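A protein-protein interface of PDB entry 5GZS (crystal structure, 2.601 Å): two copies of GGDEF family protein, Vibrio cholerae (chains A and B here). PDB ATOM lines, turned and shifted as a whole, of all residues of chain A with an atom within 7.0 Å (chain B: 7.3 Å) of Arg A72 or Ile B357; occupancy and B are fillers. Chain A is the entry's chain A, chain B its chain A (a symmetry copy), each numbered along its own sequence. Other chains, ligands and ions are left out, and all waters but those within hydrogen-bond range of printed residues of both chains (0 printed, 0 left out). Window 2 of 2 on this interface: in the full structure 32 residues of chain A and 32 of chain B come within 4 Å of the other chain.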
ATOM      1  N   PHE A  70      -8.468 -22.690  17.874  1.00  0.00           N
ATOM      2  CA  PHE A  70      -7.131 -23.243  18.103  1.00  0.00           C
ATOM      3  C   PHE A  70      -6.022 -22.277  17.730  1.00  0.00           C
ATOM      4  O   PHE A  70      -6.146 -21.513  16.760  1.00  0.00           O
ATOM      5  CB  PHE A  70      -6.926 -24.535  17.294  1.00  0.00           C
ATOM      6  CG  PHE A  70      -7.619 -25.735  17.872  1.00  0.00           C
ATOM      7  CD1 PHE A  70      -8.979 -25.913  17.698  1.00  0.00           C
ATOM      8  CD2 PHE A  70      -6.905 -26.688  18.583  1.00  0.00           C
ATOM      9  CE1 PHE A  70      -9.612 -27.009  18.236  1.00  0.00           C
ATOM     10  CE2 PHE A  70      -7.537 -27.774  19.132  1.00  0.00           C
ATOM     11  CZ  PHE A  70      -8.888 -27.944  18.952  1.00  0.00           C
ATOM     12  N   SER A  71      -4.939 -22.324  18.493  1.00  0.00           N
ATOM     13  CA  SER A  71      -3.668 -21.826  18.010  1.00  0.00           C
ATOM     14  C   SER A  71      -3.051 -22.925  17.176  1.00  0.00           C
ATOM     15  O   SER A  71      -3.519 -24.067  17.187  1.00  0.00           O
ATOM     16  CB  SER A  71      -2.713 -21.472  19.149  1.00  0.00           C
ATOM     17  OG  SER A  71      -1.943 -22.623  19.492  1.00  0.00           O
ATOM     18  N   ARG A  72      -1.980 -22.581  16.477  1.00  0.00           N
ATOM     19  CA  ARG A  72      -1.193 -23.565  15.772  1.00  0.00           C
ATOM     20  C   ARG A  72      -0.394 -24.362  16.805  1.00  0.00           C
ATOM     21  O   ARG A  72      -0.204 -23.896  17.924  1.00  0.00           O
ATOM     22  CB  ARG A  72      -0.312 -22.866  14.746  1.00  0.00           C
ATOM     23  CG  ARG A  72      -1.146 -21.990  13.816  1.00  0.00           C
ATOM     24  CD  ARG A  72      -0.411 -21.582  12.563  1.00  0.00           C
ATOM     25  NE  ARG A  72      -1.204 -21.898  11.390  1.00  0.00           N
ATOM     26  CZ  ARG A  72      -2.172 -21.126  10.925  1.00  0.00           C
ATOM     27  NH1 ARG A  72      -2.449 -19.980  11.536  1.00  0.00           N
ATOM     28  NH2 ARG A  72      -2.858 -21.499   9.850  1.00  0.00           N
ATOM     29  N   PRO A  73       0.012 -25.595  16.463  1.00  0.00           N
ATOM     30  CA  PRO A  73       0.644 -26.449  17.472  1.00  0.00           C
ATOM     31  C   PRO A  73       1.856 -25.776  18.097  1.00  0.00           C
ATOM     32  O   PRO A  73       2.596 -25.109  17.383  1.00  0.00           O
ATOM     33  CB  PRO A  73       1.031 -27.710  16.686  1.00  0.00           C
ATOM     34  CG  PRO A  73       0.759 -27.405  15.256  1.00  0.00           C
ATOM     35  CD  PRO A  73      -0.282 -26.342  15.232  1.00  0.00           C
ATOM     36  N   THR A  74       2.035 -25.925  19.409  1.00  0.00           N
ATOM     37  CA  THR A  74       3.039 -25.146  20.121  1.00  0.00           C
ATOM     38  C   THR A  74       4.107 -26.050  20.671  1.00  0.00           C
ATOM     39  O   THR A  74       5.193 -25.578  21.008  1.00  0.00           O
ATOM     40  CB  THR A  74       2.428 -24.297  21.293  1.00  0.00           C
ATOM     41  OG1 THR A  74       1.685 -25.137  22.193  1.00  0.00           O
ATOM     42  CG2 THR A  74       1.482 -23.232  20.752  1.00  0.00           C
ATOM     43  N   ASN A  75       3.804 -27.347  20.755  1.00  0.00           N
ATOM     44  CA  ASN A  75       4.703 -28.327  21.404  1.00  0.00           C
ATOM     45  C   ASN A  75       4.244 -29.769  21.258  1.00  0.00           C
ATOM     46  O   ASN A  75       3.092 -30.032  20.903  1.00  0.00           O
ATOM     47  CB  ASN A  75       4.839 -28.030  22.899  1.00  0.00           C
ATOM     48  CG  ASN A  75       3.483 -27.918  23.596  1.00  0.00           C
ATOM     49  OD1 ASN A  75       2.834 -26.861  23.563  1.00  0.00           O
ATOM     50  ND2 ASN A  75       3.035 -29.024  24.212  1.00  0.00           N
ATOM     51  N   VAL A 166       0.646 -30.739  19.439  1.00  0.00           N
ATOM     52  CA  VAL A 166      -0.395 -30.329  20.370  1.00  0.00           C
ATOM     53  C   VAL A 166      -0.492 -28.795  20.417  1.00  0.00           C
ATOM     54  O   VAL A 166       0.482 -28.107  20.112  1.00  0.00           O
ATOM     55  CB  VAL A 166      -0.085 -30.980  21.750  1.00  0.00           C
ATOM     56  CG1 VAL A 166      -1.023 -30.535  22.821  1.00  0.00           C
ATOM     57  CG2 VAL A 166      -0.056 -32.484  21.627  1.00  0.00           C
ATOM     58  N   SER A 167      -1.645 -28.237  20.761  1.00  0.00           N
ATOM     59  CA  SER A 167      -1.742 -26.779  20.716  1.00  0.00           C
ATOM     60  C   SER A 167      -2.556 -26.135  21.828  1.00  0.00           C
ATOM     61  O   SER A 167      -3.228 -26.803  22.599  1.00  0.00           O
ATOM     62  CB  SER A 167      -2.312 -26.345  19.372  1.00  0.00           C
ATOM     63  OG  SER A 167      -3.464 -27.101  19.067  1.00  0.00           O
ATOM     64  N   ILE A 168      -2.458 -24.812  21.902  1.00  0.00           N
ATOM     65  CA  ILE A 168      -3.181 -24.026  22.892  1.00  0.00           C
ATOM     66  C   ILE A 168      -4.548 -23.715  22.344  1.00  0.00           C
ATOM     67  O   ILE A 168      -4.684 -23.483  21.143  1.00  0.00           O
ATOM     68  CB  ILE A 168      -2.441 -22.719  23.232  1.00  0.00           C
ATOM     69  CG1 ILE A 168      -1.059 -23.039  23.815  1.00  0.00           C
ATOM     70  CG2 ILE A 168      -3.247 -21.894  24.205  1.00  0.00           C
ATOM     71  CD1 ILE A 168      -0.253 -21.848  24.212  1.00  0.00           C
ATOM     72  N   LEU A 179      -4.155 -14.780  21.684  1.00  0.00           N
ATOM     73  CA  LEU A 179      -3.753 -16.132  21.297  1.00  0.00           C
ATOM     74  C   LEU A 179      -2.671 -16.074  20.224  1.00  0.00           C
ATOM     75  O   LEU A 179      -1.748 -16.898  20.215  1.00  0.00           O
ATOM     76  CB  LEU A 179      -4.945 -16.941  20.795  1.00  0.00           C
ATOM     77  CG  LEU A 179      -4.611 -18.428  20.618  1.00  0.00           C
ATOM     78  CD1 LEU A 179      -4.459 -19.145  21.967  1.00  0.00           C
ATOM     79  CD2 LEU A 179      -5.614 -19.151  19.700  1.00  0.00           C
ATOM     80  N   GLU A 183       0.983 -17.563  20.588  1.00  0.00           N
ATOM     81  CA  GLU A 183       1.477 -18.466  19.566  1.00  0.00           C
ATOM     82  C   GLU A 183       2.863 -18.062  19.085  1.00  0.00           C
ATOM     83  O   GLU A 183       3.783 -18.883  19.087  1.00  0.00           O
ATOM     84  CB  GLU A 183       0.524 -18.516  18.377  1.00  0.00           C
ATOM     85  CG  GLU A 183       0.903 -19.600  17.393  1.00  0.00           C
ATOM     86  CD  GLU A 183      -0.074 -19.720  16.236  1.00  0.00           C
ATOM     87  OE1 GLU A 183       0.358 -19.543  15.077  1.00  0.00           O
ATOM     88  OE2 GLU A 183      -1.264 -20.003  16.478  1.00  0.00           O
ATOM     89  N   HIS A 187       6.801 -20.085  19.731  1.00  0.00           N
ATOM     90  CA  HIS A 187       7.594 -20.636  18.644  1.00  0.00           C
ATOM     91  C   HIS A 187       8.994 -20.065  18.636  1.00  0.00           C
ATOM     92  O   HIS A 187       9.841 -20.493  17.838  1.00  0.00           O
ATOM     93  CB  HIS A 187       6.918 -20.375  17.314  1.00  0.00           C
ATOM     94  CG  HIS A 187       5.801 -21.328  17.021  1.00  0.00           C
ATOM     95  ND1 HIS A 187       4.639 -20.951  16.380  1.00  0.00           N
ATOM     96  CD2 HIS A 187       5.671 -22.651  17.289  1.00  0.00           C
ATOM     97  CE1 HIS A 187       3.843 -21.999  16.263  1.00  0.00           C
ATOM     98  NE2 HIS A 187       4.448 -23.044  16.802  1.00  0.00           N
ATOM     99  N   LEU B 332       8.872 -31.026  14.957  1.00  0.00           N
ATOM    100  CA  LEU B 332       9.176 -29.937  14.006  1.00  0.00           C
ATOM    101  C   LEU B 332       8.143 -28.814  14.032  1.00  0.00           C
ATOM    102  O   LEU B 332       7.981 -28.061  13.064  1.00  0.00           O
ATOM    103  CB  LEU B 332       9.301 -30.468  12.579  1.00  0.00           C
ATOM    104  CG  LEU B 332      10.777 -30.511  12.189  1.00  0.00           C
ATOM    105  CD1 LEU B 332      11.588 -31.102  13.324  1.00  0.00           C
ATOM    106  CD2 LEU B 332      11.005 -31.298  10.966  1.00  0.00           C
ATOM    107  N   VAL B 333       7.488 -28.701  15.181  1.00  0.00           N
ATOM    108  CA  VAL B 333       6.330 -27.851  15.394  1.00  0.00           C
ATOM    109  C   VAL B 333       6.598 -26.389  15.064  1.00  0.00           C
ATOM    110  O   VAL B 333       5.672 -25.611  14.789  1.00  0.00           O
ATOM    111  CB  VAL B 333       5.872 -27.996  16.860  1.00  0.00           C
ATOM    112  CG1 VAL B 333       6.909 -27.404  17.817  1.00  0.00           C
ATOM    113  CG2 VAL B 333       4.533 -27.375  17.065  1.00  0.00           C
ATOM    114  N   GLU B 335       9.645 -25.585  13.119  1.00  0.00           N
ATOM    115  CA  GLU B 335      10.542 -25.514  11.971  1.00  0.00           C
ATOM    116  C   GLU B 335       9.753 -25.240  10.684  1.00  0.00           C
ATOM    117  O   GLU B 335       8.576 -25.599  10.566  1.00  0.00           O
ATOM    118  CB  GLU B 335      11.347 -26.810  11.823  1.00  0.00           C
ATOM    119  CG  GLU B 335      12.280 -27.119  12.982  1.00  0.00           C
ATOM    120  CD  GLU B 335      13.545 -26.269  12.988  1.00  0.00           C
ATOM    121  OE1 GLU B 335      14.264 -26.291  14.010  1.00  0.00           O
ATOM    122  OE2 GLU B 335      13.833 -25.596  11.979  1.00  0.00           O
ATOM    123  N   ARG B 336      10.411 -24.609   9.721  1.00  0.00           N
ATOM    124  CA  ARG B 336       9.779 -24.304   8.451  1.00  0.00           C
ATOM    125  C   ARG B 336       9.846 -25.514   7.533  1.00  0.00           C
ATOM    126  O   ARG B 336      10.933 -25.925   7.127  1.00  0.00           O
ATOM    127  CB  ARG B 336      10.452 -23.103   7.790  1.00  0.00           C
ATOM    128  CG  ARG B 336      10.339 -21.803   8.572  1.00  0.00           C
ATOM    129  CD  ARG B 336      10.746 -20.616   7.710  1.00  0.00           C
ATOM    130  NE  ARG B 336      11.834 -19.854   8.303  1.00  0.00           N
ATOM    131  CZ  ARG B 336      13.115 -19.947   7.950  1.00  0.00           C
ATOM    132  NH1 ARG B 336      13.503 -20.774   6.986  1.00  0.00           N
ATOM    133  NH2 ARG B 336      14.018 -19.194   8.577  1.00  0.00           N
ATOM    134  N   ILE B 337       8.697 -26.100   7.220  1.00  0.00           N
ATOM    135  CA  ILE B 337       8.693 -27.261   6.354  1.00  0.00           C
ATOM    136  C   ILE B 337       8.137 -26.905   4.998  1.00  0.00           C
ATOM    137  O   ILE B 337       7.051 -26.328   4.883  1.00  0.00           O
ATOM    138  CB  ILE B 337       7.888 -28.428   6.939  1.00  0.00           C
ATOM    139  CG1 ILE B 337       8.612 -29.020   8.162  1.00  0.00           C
ATOM    140  CG2 ILE B 337       7.713 -29.507   5.894  1.00  0.00           C
ATOM    141  CD1 ILE B 337       7.707 -29.755   9.090  1.00  0.00           C
ATOM    142  N   GLY B 338       8.885 -27.242   3.961  1.00  0.00           N
ATOM    143  CA  GLY B 338       8.430 -26.952   2.622  1.00  0.00           C
ATOM    144  C   GLY B 338       7.824 -28.156   1.947  1.00  0.00           C
ATOM    145  O   GLY B 338       8.448 -29.223   1.896  1.00  0.00           O
ATOM    146  N   LEU B 353       0.825 -33.170  11.193  1.00  0.00           N
ATOM    147  CA  LEU B 353       1.050 -31.946  11.991  1.00  0.00           C
ATOM    148  C   LEU B 353      -0.101 -30.948  11.839  1.00  0.00           C
ATOM    149  O   LEU B 353       0.048 -29.903  11.192  1.00  0.00           O
ATOM    150  CB  LEU B 353       2.370 -31.285  11.597  1.00  0.00           C
ATOM    151  CG  LEU B 353       3.511 -32.269  11.318  1.00  0.00           C
ATOM    152  CD1 LEU B 353       4.642 -31.567  10.584  1.00  0.00           C
ATOM    153  CD2 LEU B 353       3.998 -32.882  12.584  1.00  0.00           C
ATOM    154  N   PRO B 354      -1.244 -31.260  12.466  1.00  0.00           N
ATOM    155  CA  PRO B 354      -2.512 -30.560  12.238  1.00  0.00           C
ATOM    156  C   PRO B 354      -2.432 -29.060  12.484  1.00  0.00           C
ATOM    157  O   PRO B 354      -1.754 -28.635  13.418  1.00  0.00           O
ATOM    158  CB  PRO B 354      -3.460 -31.217  13.251  1.00  0.00           C
ATOM    159  CG  PRO B 354      -2.812 -32.519  13.621  1.00  0.00           C
ATOM    160  CD  PRO B 354      -1.350 -32.273  13.533  1.00  0.00           C
ATOM    161  N   ASN B 355      -3.100 -28.279  11.637  1.00  0.00           N
ATOM    162  CA  ASN B 355      -3.249 -26.830  11.826  1.00  0.00           C
ATOM    163  C   ASN B 355      -1.929 -26.056  11.836  1.00  0.00           C
ATOM    164  O   ASN B 355      -1.870 -24.897  12.246  1.00  0.00           O
ATOM    165  CB  ASN B 355      -4.002 -26.560  13.126  1.00  0.00           C
ATOM    166  CG  ASN B 355      -4.694 -25.238  13.116  1.00  0.00           C
ATOM    167  OD1 ASN B 355      -5.059 -24.733  12.050  1.00  0.00           O
ATOM    168  ND2 ASN B 355      -4.861 -24.642  14.294  1.00  0.00           N
ATOM    169  N   LYS B 356      -0.870 -26.725  11.399  1.00  0.00           N
ATOM    170  CA  LYS B 356       0.468 -26.152  11.344  1.00  0.00           C
ATOM    171  C   LYS B 356       0.685 -25.497   9.981  1.00  0.00           C
ATOM    172  O   LYS B 356       0.188 -25.991   8.961  1.00  0.00           O
ATOM    173  CB  LYS B 356       1.517 -27.243  11.595  1.00  0.00           C
ATOM    174  CG  LYS B 356       2.963 -26.839  11.359  1.00  0.00           C
ATOM    175  CD  LYS B 356       3.866 -28.068  11.233  1.00  0.00           C
ATOM    176  CE  LYS B 356       5.322 -27.680  11.067  1.00  0.00           C
ATOM    177  NZ  LYS B 356       5.584 -26.330  11.651  1.00  0.00           N
ATOM    178  N   ILE B 357       1.419 -24.389   9.952  1.00  0.00           N
ATOM    179  CA  ILE B 357       1.745 -23.789   8.672  1.00  0.00           C
ATOM    180  C   ILE B 357       2.801 -24.600   7.952  1.00  0.00           C
ATOM    181  O   ILE B 357       3.909 -24.812   8.467  1.00  0.00           O
ATOM    182  CB  ILE B 357       2.255 -22.359   8.796  1.00  0.00           C
ATOM    183  CG1 ILE B 357       1.142 -21.457   9.298  1.00  0.00           C
ATOM    184  CG2 ILE B 357       2.628 -21.852   7.405  1.00  0.00           C
ATOM    185  CD1 ILE B 357      -0.054 -21.462   8.348  1.00  0.00           C
ATOM    186  N   LEU B 358       2.429 -25.074   6.769  1.00  0.00           N
ATOM    187  CA  LEU B 358       3.375 -25.620   5.822  1.00  0.00           C
ATOM    188  C   LEU B 358       3.597 -24.532   4.780  1.00  0.00           C
ATOM    189  O   LEU B 358       2.712 -23.704   4.558  1.00  0.00           O
ATOM    190  CB  LEU B 358       2.842 -26.908   5.188  1.00  0.00           C
ATOM    191  CG  LEU B 358       2.194 -27.934   6.126  1.00  0.00           C
ATOM    192  CD1 LEU B 358       1.496 -29.056   5.334  1.00  0.00           C
ATOM    193  CD2 LEU B 358       3.241 -28.501   7.032  1.00  0.00           C
ATOM    194  N   PHE B 359       4.780 -24.503   4.170  1.00  0.00           N
ATOM    195  CA  PHE B 359       5.049 -23.590   3.060  1.00  0.00           C
ATOM    196  C   PHE B 359       4.862 -24.376   1.773  1.00  0.00           C
ATOM    197  O   PHE B 359       5.438 -25.458   1.625  1.00  0.00           O
ATOM    198  CB  PHE B 359       6.457 -23.002   3.145  1.00  0.00           C
ATOM    199  CG  PHE B 359       6.664 -22.102   4.327  1.00  0.00           C
ATOM    200  CD1 PHE B 359       7.074 -22.610   5.554  1.00  0.00           C
ATOM    201  CD2 PHE B 359       6.444 -20.741   4.212  1.00  0.00           C
ATOM    202  CE1 PHE B 359       7.261 -21.772   6.641  1.00  0.00           C
ATOM    203  CE2 PHE B 359       6.626 -19.903   5.280  1.00  0.00           C
ATOM    204  CZ  PHE B 359       7.036 -20.409   6.501  1.00  0.00           C
ATOM    205  N   SER B 360       4.047 -23.860   0.857  1.00  0.00           N
ATOM    206  CA  SER B 360       3.732 -24.618  -0.350  1.00  0.00           C
ATOM    207  C   SER B 360       4.463 -24.078  -1.567  1.00  0.00           C
ATOM    208  O   SER B 360       4.742 -22.883  -1.663  1.00  0.00           O
ATOM    209  CB  SER B 360       2.222 -24.633  -0.610  1.00  0.00           C
ATOM    210  OG  SER B 360       1.490 -24.701   0.602  1.00  0.00           O
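The backbone carbonyl oxygen of Ser A71 sits at hydrogen-bond distance from the side-chain amide nitrogen of Asn B355 (3.2 Å).
The backbone carbonyl oxygen of Asn B355 sits at hydrogen-bond distance from the guanidinium group of Arg A72, 3.2 Å away.
O of Val B333 is in hydrogen-bond range of NE2 of His A187, at 3.5 Å.
The backbone NH of Arg A72 lies within hydrogen-bond range of the side-chain carboxylate of Glu A183 (2.7 Å).
NZ of Lys B356 lies within hydrogen-bond range of O of Leu B332, 3.3 Å away.
O of Pro A73 lies within hydrogen-bond range of NE2 of His A187 (2.8 Å).
The backbone NH of Ser A71 sits at hydrogen-bond distance from the backbone carbonyl oxygen of Ile A168 (2.9 Å).
O of Asn A75 lies within hydrogen-bond range of N of Val A166, at 2.9 Å.
N of Thr A74 sits at hydrogen-bond distance from O of Val A166, 2.8 Å away.
Among the printed residues, pairs that only touch across the chains: Pro A73 with Val B333 (3.0 Å), Arg A72 with Ile B357 (3.2 Å), Pro A73 with Pro B354 (3.3 Å), Phe A70 with Asn B355 (3.6 Å), Pro A73 with Asn B355 (3.7 Å), Thr A74 with Val B333 (3.7 Å), Pro A73 with Lys B356 (3.7 Å) and Asn A75 with Val B333 (3.8 Å).
Of chain B, only Asn B355 and Ile B357 come within 4 Å of Arg A72.
Printed residues of chain B within 4 Å of Asn A75: Val B333 (3.8 Å).
Leu A179 touches none of the printed residues of chain B.
Of the printed residues of chain A, Asn B355 touches Phe A70 (3.6 Å), Ser A71 (3.2 Å), Arg A72 (3.2 Å) and Pro A73 (3.7 Å).
Ile B357 touches just one residue of chain A: Arg A72.
Leu B358 touches none of the printed residues of chain A.
The nearest residue of chain A that does not touch Ile B357 is Pro A73 (5.9 Å).
Of the 14 printed residues of chain B, 5 touch a printed residue of chain A.
Along chain B the printed residues that touch a printed residue of chain A span positions 333 to 357.
Among the printed residues, no Asp or Glu carboxylate lies within 4 Å of a Lys or Arg side-chain nitrogen of the other chain.
No position is printed for both chains.
Of the 11 pairs that touch across the chains among the printed residues, none has its exchanged pair printed and touching as well.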
